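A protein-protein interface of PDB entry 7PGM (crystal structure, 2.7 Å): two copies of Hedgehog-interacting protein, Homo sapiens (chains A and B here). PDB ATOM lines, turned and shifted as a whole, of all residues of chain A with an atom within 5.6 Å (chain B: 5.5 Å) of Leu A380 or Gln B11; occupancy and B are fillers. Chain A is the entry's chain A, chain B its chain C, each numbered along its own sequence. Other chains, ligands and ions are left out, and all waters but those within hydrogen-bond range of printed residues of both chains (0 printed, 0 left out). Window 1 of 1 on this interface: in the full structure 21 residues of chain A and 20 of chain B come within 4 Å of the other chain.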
ATOM      1  N   GLN A  11     -28.856 -16.278   5.774  1.00  0.00           N
ATOM      2  CA  GLN A  11     -28.475 -17.641   6.127  1.00  0.00           C
ATOM      3  C   GLN A  11     -29.542 -18.302   6.987  1.00  0.00           C
ATOM      4  O   GLN A  11     -29.911 -17.777   8.044  1.00  0.00           O
ATOM      5  CB  GLN A  11     -27.141 -17.656   6.876  1.00  0.00           C
ATOM      6  CG  GLN A  11     -26.637 -19.051   7.192  1.00  0.00           C
ATOM      7  CD  GLN A  11     -25.782 -19.608   6.078  1.00  0.00           C
ATOM      8  OE1 GLN A  11     -26.081 -20.667   5.524  1.00  0.00           O
ATOM      9  NE2 GLN A  11     -24.710 -18.896   5.738  1.00  0.00           N
ATOM     10  N   GLN A 292     -20.282  -9.010  13.573  1.00  0.00           N
ATOM     11  CA  GLN A 292     -19.823  -9.691  12.369  1.00  0.00           C
ATOM     12  C   GLN A 292     -19.634  -8.713  11.220  1.00  0.00           C
ATOM     13  O   GLN A 292     -18.656  -8.812  10.470  1.00  0.00           O
ATOM     14  CB  GLN A 292     -20.800 -10.799  11.979  1.00  0.00           C
ATOM     15  CG  GLN A 292     -20.230 -11.785  10.976  1.00  0.00           C
ATOM     16  CD  GLN A 292     -20.624 -11.456   9.545  1.00  0.00           C
ATOM     17  OE1 GLN A 292     -21.695 -10.900   9.295  1.00  0.00           O
ATOM     18  NE2 GLN A 292     -19.758 -11.803   8.598  1.00  0.00           N
ATOM     19  N   SER A 333     -23.643 -20.945   0.734  1.00  0.00           N
ATOM     20  CA  SER A 333     -24.812 -21.273   1.547  1.00  0.00           C
ATOM     21  C   SER A 333     -25.607 -20.025   1.887  1.00  0.00           C
ATOM     22  O   SER A 333     -26.821 -20.097   2.105  1.00  0.00           O
ATOM     23  CB  SER A 333     -24.376 -21.964   2.836  1.00  0.00           C
ATOM     24  OG  SER A 333     -23.336 -22.894   2.594  1.00  0.00           O
ATOM     25  N   CYS A 334     -24.934 -18.885   1.967  1.00  0.00           N
ATOM     26  CA  CYS A 334     -25.568 -17.622   2.302  1.00  0.00           C
ATOM     27  C   CYS A 334     -26.148 -17.031   1.022  1.00  0.00           C
ATOM     28  O   CYS A 334     -25.404 -16.733   0.083  1.00  0.00           O
ATOM     29  CB  CYS A 334     -24.521 -16.701   2.924  1.00  0.00           C
ATOM     30  SG  CYS A 334     -25.126 -15.421   3.978  1.00  0.00           S
ATOM     31  N   VAL A 374     -26.105 -11.803   7.175  1.00  0.00           N
ATOM     32  CA  VAL A 374     -24.661 -11.961   7.177  1.00  0.00           C
ATOM     33  C   VAL A 374     -24.042 -10.920   6.257  1.00  0.00           C
ATOM     34  O   VAL A 374     -24.648 -10.483   5.275  1.00  0.00           O
ATOM     35  CB  VAL A 374     -24.280 -13.395   6.747  1.00  0.00           C
ATOM     36  CG1 VAL A 374     -22.767 -13.632   6.834  1.00  0.00           C
ATOM     37  CG2 VAL A 374     -25.036 -14.405   7.586  1.00  0.00           C
ATOM     38  N   ARG A 378     -17.031 -10.119   5.403  1.00  0.00           N
ATOM     39  CA  ARG A 378     -16.335 -10.330   6.659  1.00  0.00           C
ATOM     40  C   ARG A 378     -16.371 -11.800   7.058  1.00  0.00           C
ATOM     41  O   ARG A 378     -17.276 -12.537   6.654  1.00  0.00           O
ATOM     42  CB  ARG A 378     -16.957  -9.493   7.780  1.00  0.00           C
ATOM     43  CG  ARG A 378     -16.694  -8.017   7.647  1.00  0.00           C
ATOM     44  CD  ARG A 378     -15.632  -7.578   8.624  1.00  0.00           C
ATOM     45  NE  ARG A 378     -16.036  -7.821  10.005  1.00  0.00           N
ATOM     46  CZ  ARG A 378     -15.229  -7.667  11.048  1.00  0.00           C
ATOM     47  NH1 ARG A 378     -13.975  -7.274  10.858  1.00  0.00           N
ATOM     48  NH2 ARG A 378     -15.669  -7.901  12.277  1.00  0.00           N
ATOM     49  N   PRO A 379     -15.393 -12.253   7.844  1.00  0.00           N
ATOM     50  CA  PRO A 379     -15.441 -13.620   8.371  1.00  0.00           C
ATOM     51  C   PRO A 379     -16.710 -13.874   9.168  1.00  0.00           C
ATOM     52  O   PRO A 379     -17.358 -12.958   9.681  1.00  0.00           O
ATOM     53  CB  PRO A 379     -14.204 -13.696   9.273  1.00  0.00           C
ATOM     54  CG  PRO A 379     -13.289 -12.657   8.757  1.00  0.00           C
ATOM     55  CD  PRO A 379     -14.159 -11.554   8.238  1.00  0.00           C
ATOM     56  N   LEU A 380     -17.060 -15.155   9.270  1.00  0.00           N
ATOM     57  CA  LEU A 380     -18.199 -15.538  10.093  1.00  0.00           C
ATOM     58  C   LEU A 380     -17.890 -15.342  11.570  1.00  0.00           C
ATOM     59  O   LEU A 380     -18.757 -14.921  12.345  1.00  0.00           O
ATOM     60  CB  LEU A 380     -18.576 -16.986   9.810  1.00  0.00           C
ATOM     61  CG  LEU A 380     -19.466 -17.169   8.587  1.00  0.00           C
ATOM     62  CD1 LEU A 380     -19.888 -18.624   8.489  1.00  0.00           C
ATOM     63  CD2 LEU A 380     -20.662 -16.231   8.662  1.00  0.00           C
ATOM     64  N   MET A 381     -16.663 -15.662  11.980  1.00  0.00           N
ATOM     65  CA  MET A 381     -16.194 -15.438  13.346  1.00  0.00           C
ATOM     66  C   MET A 381     -14.901 -14.636  13.293  1.00  0.00           C
ATOM     67  O   MET A 381     -13.803 -15.188  13.458  1.00  0.00           O
ATOM     68  CB  MET A 381     -15.995 -16.753  14.101  1.00  0.00           C
ATOM     69  CG  MET A 381     -15.926 -16.578  15.613  1.00  0.00           C
ATOM     70  SD  MET A 381     -17.188 -15.438  16.239  1.00  0.00           S
ATOM     71  CE  MET A 381     -18.714 -16.302  15.843  1.00  0.00           C
ATOM     72  N   PRO A 382     -14.994 -13.327  13.072  1.00  0.00           N
ATOM     73  CA  PRO A 382     -13.804 -12.480  13.184  1.00  0.00           C
ATOM     74  C   PRO A 382     -13.198 -12.620  14.569  1.00  0.00           C
ATOM     75  O   PRO A 382     -13.902 -12.874  15.550  1.00  0.00           O
ATOM     76  CB  PRO A 382     -14.346 -11.063  12.951  1.00  0.00           C
ATOM     77  CG  PRO A 382     -15.660 -11.262  12.266  1.00  0.00           C
ATOM     78  CD  PRO A 382     -16.209 -12.534  12.815  1.00  0.00           C
ATOM     79  N   CYS B   9     -15.930 -25.224  10.208  1.00  0.00           N
ATOM     80  CA  CYS B   9     -17.336 -25.409  10.514  1.00  0.00           C
ATOM     81  C   CYS B   9     -18.071 -25.929   9.287  1.00  0.00           C
ATOM     82  O   CYS B   9     -17.571 -25.882   8.159  1.00  0.00           O
ATOM     83  CB  CYS B   9     -18.004 -24.122  11.017  1.00  0.00           C
ATOM     84  SG  CYS B   9     -17.909 -22.773   9.879  1.00  0.00           S
ATOM     85  N   ILE B  10     -19.274 -26.430   9.542  1.00  0.00           N
ATOM     86  CA  ILE B  10     -20.095 -27.124   8.563  1.00  0.00           C
ATOM     87  C   ILE B  10     -21.381 -26.338   8.378  1.00  0.00           C
ATOM     88  O   ILE B  10     -22.072 -26.034   9.358  1.00  0.00           O
ATOM     89  CB  ILE B  10     -20.393 -28.560   9.033  1.00  0.00           C
ATOM     90  CG1 ILE B  10     -19.111 -29.226   9.517  1.00  0.00           C
ATOM     91  CG2 ILE B  10     -20.944 -29.370   7.934  1.00  0.00           C
ATOM     92  CD1 ILE B  10     -18.038 -29.303   8.447  1.00  0.00           C
ATOM     93  N   GLN B  11     -21.692 -25.986   7.134  1.00  0.00           N
ATOM     94  CA  GLN B  11     -22.893 -25.219   6.844  1.00  0.00           C
ATOM     95  C   GLN B  11     -23.764 -26.053   5.911  1.00  0.00           C
ATOM     96  O   GLN B  11     -23.299 -26.497   4.858  1.00  0.00           O
ATOM     97  CB  GLN B  11     -22.534 -23.863   6.234  1.00  0.00           C
ATOM     98  CG  GLN B  11     -23.656 -22.852   6.241  1.00  0.00           C
ATOM     99  CD  GLN B  11     -23.178 -21.517   6.809  1.00  0.00           C
ATOM    100  OE1 GLN B  11     -23.721 -21.010   7.795  1.00  0.00           O
ATOM    101  NE2 GLN B  11     -22.170 -20.932   6.166  1.00  0.00           N
ATOM    102  N   GLU B  12     -25.017 -26.279   6.300  1.00  0.00           N
ATOM    103  CA  GLU B  12     -25.919 -27.085   5.486  1.00  0.00           C
ATOM    104  C   GLU B  12     -26.288 -26.336   4.212  1.00  0.00           C
ATOM    105  O   GLU B  12     -26.689 -25.169   4.259  1.00  0.00           O
ATOM    106  CB  GLU B  12     -27.172 -27.443   6.288  1.00  0.00           C
ATOM    107  CG  GLU B  12     -28.166 -28.381   5.592  1.00  0.00           C
ATOM    108  CD  GLU B  12     -29.317 -28.795   6.506  1.00  0.00           C
ATOM    109  OE1 GLU B  12     -29.071 -29.020   7.711  1.00  0.00           O
ATOM    110  OE2 GLU B  12     -30.467 -28.888   6.023  1.00  0.00           O
ATOM    111  N   VAL B  13     -26.145 -27.009   3.072  1.00  0.00           N
ATOM    112  CA  VAL B  13     -26.417 -26.417   1.764  1.00  0.00           C
ATOM    113  C   VAL B  13     -27.739 -26.896   1.182  1.00  0.00           C
ATOM    114  O   VAL B  13     -28.594 -26.086   0.821  1.00  0.00           O
ATOM    115  CB  VAL B  13     -25.254 -26.715   0.791  1.00  0.00           C
ATOM    116  CG1 VAL B  13     -25.534 -26.073  -0.571  1.00  0.00           C
ATOM    117  CG2 VAL B  13     -23.931 -26.247   1.363  1.00  0.00           C
ATOM    118  N   SER B 331     -19.356 -21.733  14.975  1.00  0.00           N
ATOM    119  CA  SER B 331     -19.141 -20.292  14.886  1.00  0.00           C
ATOM    120  C   SER B 331     -20.479 -19.729  14.428  1.00  0.00           C
ATOM    121  O   SER B 331     -20.770 -19.692  13.228  1.00  0.00           O
ATOM    122  CB  SER B 331     -18.003 -19.939  13.927  1.00  0.00           C
ATOM    123  OG  SER B 331     -16.830 -20.684  14.216  1.00  0.00           O
ATOM    124  N   SER B 333     -23.966 -19.438  13.171  1.00  0.00           N
ATOM    125  CA  SER B 333     -24.817 -20.312  12.371  1.00  0.00           C
ATOM    126  C   SER B 333     -24.043 -21.496  11.812  1.00  0.00           C
ATOM    127  O   SER B 333     -24.636 -22.534  11.507  1.00  0.00           O
ATOM    128  CB  SER B 333     -25.461 -19.517  11.240  1.00  0.00           C
ATOM    129  OG  SER B 333     -25.911 -18.262  11.715  1.00  0.00           O
ATOM    130  N   CYS B 334     -22.739 -21.336  11.623  1.00  0.00           N
ATOM    131  CA  CYS B 334     -21.890 -22.381  11.069  1.00  0.00           C
ATOM    132  C   CYS B 334     -21.486 -23.341  12.182  1.00  0.00           C
ATOM    133  O   CYS B 334     -20.873 -22.922  13.169  1.00  0.00           O
ATOM    134  CB  CYS B 334     -20.666 -21.728  10.435  1.00  0.00           C
ATOM    135  SG  CYS B 334     -19.819 -22.702   9.211  1.00  0.00           S
ATOM    136  N   ARG B 335     -21.802 -24.624  12.031  1.00  0.00           N
ATOM    137  CA  ARG B 335     -21.781 -25.525  13.175  1.00  0.00           C
ATOM    138  C   ARG B 335     -20.662 -26.554  13.083  1.00  0.00           C
ATOM    139  O   ARG B 335     -20.212 -26.922  11.995  1.00  0.00           O
ATOM    140  CB  ARG B 335     -23.133 -26.229  13.327  1.00  0.00           C
ATOM    141  CG  ARG B 335     -24.301 -25.258  13.280  1.00  0.00           C
ATOM    142  CD  ARG B 335     -25.546 -25.821  13.937  1.00  0.00           C
ATOM    143  NE  ARG B 335     -26.614 -24.827  14.016  1.00  0.00           N
ATOM    144  CZ  ARG B 335     -27.559 -24.660  13.098  1.00  0.00           C
ATOM    145  NH1 ARG B 335     -27.582 -25.424  12.014  1.00  0.00           N
ATOM    146  NH2 ARG B 335     -28.486 -23.726  13.267  1.00  0.00           N
ATOM    147  N   LEU B 370     -26.278 -32.309   2.169  1.00  0.00           N
ATOM    148  CA  LEU B 370     -25.031 -31.815   1.593  1.00  0.00           C
ATOM    149  C   LEU B 370     -24.501 -30.680   2.458  1.00  0.00           C
ATOM    150  O   LEU B 370     -25.176 -29.662   2.642  1.00  0.00           O
ATOM    151  CB  LEU B 370     -25.240 -31.326   0.160  1.00  0.00           C
ATOM    152  CG  LEU B 370     -24.041 -30.606  -0.463  1.00  0.00           C
ATOM    153  CD1 LEU B 370     -22.957 -31.594  -0.858  1.00  0.00           C
ATOM    154  CD2 LEU B 370     -24.459 -29.750  -1.651  1.00  0.00           C
ATOM    155  N   TYR B 371     -23.280 -30.830   2.944  1.00  0.00           N
ATOM    156  CA  TYR B 371     -22.683 -29.872   3.855  1.00  0.00           C
ATOM    157  C   TYR B 371     -21.443 -29.245   3.236  1.00  0.00           C
ATOM    158  O   TYR B 371     -20.627 -29.941   2.627  1.00  0.00           O
ATOM    159  CB  TYR B 371     -22.306 -30.557   5.153  1.00  0.00           C
ATOM    160  CG  TYR B 371     -23.464 -30.909   6.056  1.00  0.00           C
ATOM    161  CD1 TYR B 371     -24.098 -29.932   6.808  1.00  0.00           C
ATOM    162  CD2 TYR B 371     -23.883 -32.223   6.203  1.00  0.00           C
ATOM    163  CE1 TYR B 371     -25.132 -30.242   7.654  1.00  0.00           C
ATOM    164  CE2 TYR B 371     -24.921 -32.547   7.057  1.00  0.00           C
ATOM    165  CZ  TYR B 371     -25.541 -31.550   7.782  1.00  0.00           C
ATOM    166  OH  TYR B 371     -26.577 -31.858   8.635  1.00  0.00           O
ATOM    167  N   LYS B 372     -21.293 -27.934   3.409  1.00  0.00           N
ATOM    168  CA  LYS B 372     -20.098 -27.228   2.966  1.00  0.00           C
ATOM    169  C   LYS B 372     -19.159 -26.987   4.137  1.00  0.00           C
ATOM    170  O   LYS B 372     -19.597 -26.666   5.247  1.00  0.00           O
ATOM    171  CB  LYS B 372     -20.452 -25.898   2.302  1.00  0.00           C
ATOM    172  CG  LYS B 372     -19.276 -25.194   1.627  1.00  0.00           C
ATOM    173  CD  LYS B 372     -19.789 -24.340   0.473  1.00  0.00           C
ATOM    174  CE  LYS B 372     -18.813 -23.263   0.075  1.00  0.00           C
ATOM    175  NZ  LYS B 372     -19.205 -22.712  -1.251  1.00  0.00           N
ATOM    176  N   ILE B 373     -17.868 -27.158   3.885  1.00  0.00           N
ATOM    177  CA  ILE B 373     -16.839 -26.856   4.870  1.00  0.00           C
ATOM    178  C   ILE B 373     -16.434 -25.396   4.723  1.00  0.00           C
ATOM    179  O   ILE B 373     -16.124 -24.932   3.619  1.00  0.00           O
ATOM    180  CB  ILE B 373     -15.631 -27.792   4.713  1.00  0.00           C
ATOM    181  CG1 ILE B 373     -16.005 -29.224   5.109  1.00  0.00           C
ATOM    182  CG2 ILE B 373     -14.466 -27.297   5.539  1.00  0.00           C
ATOM    183  CD1 ILE B 373     -14.893 -30.244   4.879  1.00  0.00           C
ATOM    184  N   VAL B 374     -16.448 -24.667   5.834  1.00  0.00           N
ATOM    185  CA  VAL B 374     -16.185 -23.236   5.830  1.00  0.00           C
ATOM    186  C   VAL B 374     -14.995 -22.971   6.741  1.00  0.00           C
ATOM    187  O   VAL B 374     -14.760 -23.696   7.713  1.00  0.00           O
ATOM    188  CB  VAL B 374     -17.427 -22.430   6.281  1.00  0.00           C
ATOM    189  CG1 VAL B 374     -17.173 -20.931   6.196  1.00  0.00           C
ATOM    190  CG2 VAL B 374     -18.637 -22.812   5.447  1.00  0.00           C
ATOM    191  N   PRO B 376     -14.108 -20.261   9.200  1.00  0.00           N
ATOM    192  CA  PRO B 376     -14.710 -19.072   9.813  1.00  0.00           C
ATOM    193  C   PRO B 376     -13.713 -17.966  10.073  1.00  0.00           C
ATOM    194  O   PRO B 376     -14.131 -16.840  10.364  1.00  0.00           O
ATOM    195  CB  PRO B 376     -15.295 -19.609  11.119  1.00  0.00           C
ATOM    196  CG  PRO B 376     -14.443 -20.778  11.449  1.00  0.00           C
ATOM    197  CD  PRO B 376     -13.960 -21.368  10.157  1.00  0.00           C
ATOM    198  N   ARG B 378     -12.054 -16.718   7.750  1.00  0.00           N
ATOM    199  CA  ARG B 378     -12.050 -16.002   6.486  1.00  0.00           C
ATOM    200  C   ARG B 378     -13.460 -15.589   6.072  1.00  0.00           C
ATOM    201  O   ARG B 378     -14.445 -16.213   6.482  1.00  0.00           O
ATOM    202  CB  ARG B 378     -11.431 -16.866   5.381  1.00  0.00           C
ATOM    203  CG  ARG B 378      -9.945 -17.056   5.531  1.00  0.00           C
ATOM    204  CD  ARG B 378      -9.206 -16.163   4.563  1.00  0.00           C
ATOM    205  NE  ARG B 378      -9.559 -16.477   3.186  1.00  0.00           N
ATOM    206  CZ  ARG B 378      -9.189 -15.751   2.138  1.00  0.00           C
ATOM    207  NH1 ARG B 378      -8.452 -14.660   2.310  1.00  0.00           N
ATOM    208  NH2 ARG B 378      -9.557 -16.116   0.918  1.00  0.00           N
ATOM    209  N   PRO B 379     -13.584 -14.535   5.265  1.00  0.00           N
ATOM    210  CA  PRO B 379     -14.895 -14.159   4.720  1.00  0.00           C
ATOM    211  C   PRO B 379     -15.529 -15.288   3.923  1.00  0.00           C
ATOM    212  O   PRO B 379     -14.853 -16.186   3.414  1.00  0.00           O
ATOM    213  CB  PRO B 379     -14.574 -12.969   3.806  1.00  0.00           C
ATOM    214  CG  PRO B 379     -13.295 -12.423   4.321  1.00  0.00           C
ATOM    215  CD  PRO B 379     -12.525 -13.592   4.860  1.00  0.00           C
ATOM    216  N   LEU B 380     -16.860 -15.230   3.811  1.00  0.00           N
ATOM    217  CA  LEU B 380     -17.565 -16.202   2.982  1.00  0.00           C
ATOM    218  C   LEU B 380     -17.315 -15.955   1.500  1.00  0.00           C
ATOM    219  O   LEU B 380     -17.162 -16.905   0.725  1.00  0.00           O
ATOM    220  CB  LEU B 380     -19.063 -16.181   3.285  1.00  0.00           C
ATOM    221  CG  LEU B 380     -19.497 -17.063   4.451  1.00  0.00           C
ATOM    222  CD1 LEU B 380     -21.003 -17.069   4.568  1.00  0.00           C
ATOM    223  CD2 LEU B 380     -18.976 -18.465   4.255  1.00  0.00           C
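Of the printed residues of chain B, Met A381 touches Ser B331 and Pro B376.
Printed residues of chain A within 4 Å of Pro B376: Pro A379, Leu A380 and Met A381.
Cys B9 touches none of the printed residues of chain A.
Pro A382 touches none of the printed residues of chain B.
The nearest printed residue of chain B that does not touch Leu A380 is Leu B380 (4.1 Å).
The nearest printed residue of chain A that does not touch Gln B11 is Cys A334 (5.4 Å).
The nearest printed residue of chain A that does not touch Val B13 is Gln A11 (6.8 Å).
The side-chain amide oxygen of Gln B11 sits close to the side-chain amide nitrogen of Gln A11 (3.1 Å).
N of Met A381 is in hydrogen-bond range of O of Pro B376.
The backbone carbonyl oxygen (O) of Gln B11 is in hydrogen-bond range of the backbone NH (N) of Lys B372, 2.9 Å away.
The backbone carbonyl oxygen of Gln A292 lies within hydrogen-bond range of the guanidinium group of Arg A378, at 2.8 Å.
The backbone carbonyl oxygen of Pro A379 is in hydrogen-bond range of the side-chain amide nitrogen of Gln A292 (2.9 Å).
The side-chain sulfur of Cys B334 forms a disulfide with the side-chain sulfur of Cys B9, at 2.0 Å.
The backbone NH of Ile B10 is in hydrogen-bond range of the side-chain sulfur of Cys B334 (3.8 Å).
The backbone NH of Val B13 is in hydrogen-bond range of the backbone carbonyl oxygen of Leu B370 (2.9 Å).
Ser A333 touches Val B13.
CD1 of Leu B380 touches CB of Cys A334, 3.9 Å away.
Pro B379 touches Arg A378.
O of Arg A378 touches N of Leu B380, 3.9 Å away.
Pro A379 touches Arg B378 (CA to O, 3.4 Å).
CD1 of Leu A380 touches NE2 of Gln B11, 3.99 Å away.
CD1 of Leu A380 touches CB of Cys B334, at 3.7 Å.
O of Pro B376 touches N of Leu A380, at 3.6 Å.
Leu A380 touches Arg B378.
Ser B331 touches Met A381.
Gln A11 touches its own counterpart, Gln B11.
Cys A334 touches Leu B380, and with the chains exchanged Leu A380 touches Cys B334.
Arg A378 touches Pro B379, and with the chains exchanged Pro A379 touches Arg B378.
Pro A379 touches its own counterpart, Pro B379.
7 positions are printed for both chains.
Of the 15 pairs that touch across the chains among the printed residues, 8 have their exchanged pair printed and touching as well.
Hydrophobic or aromatic side chains of chain A within 4 Å of the printed part of chain B: Pro A379, Leu A380 and Met A381.
Hydrophobic or aromatic side chains of chain B that line the printed part of chain A: Val B13, Pro B379 and Leu B380.
Among the printed residues, 15 pairs touch across the chains.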
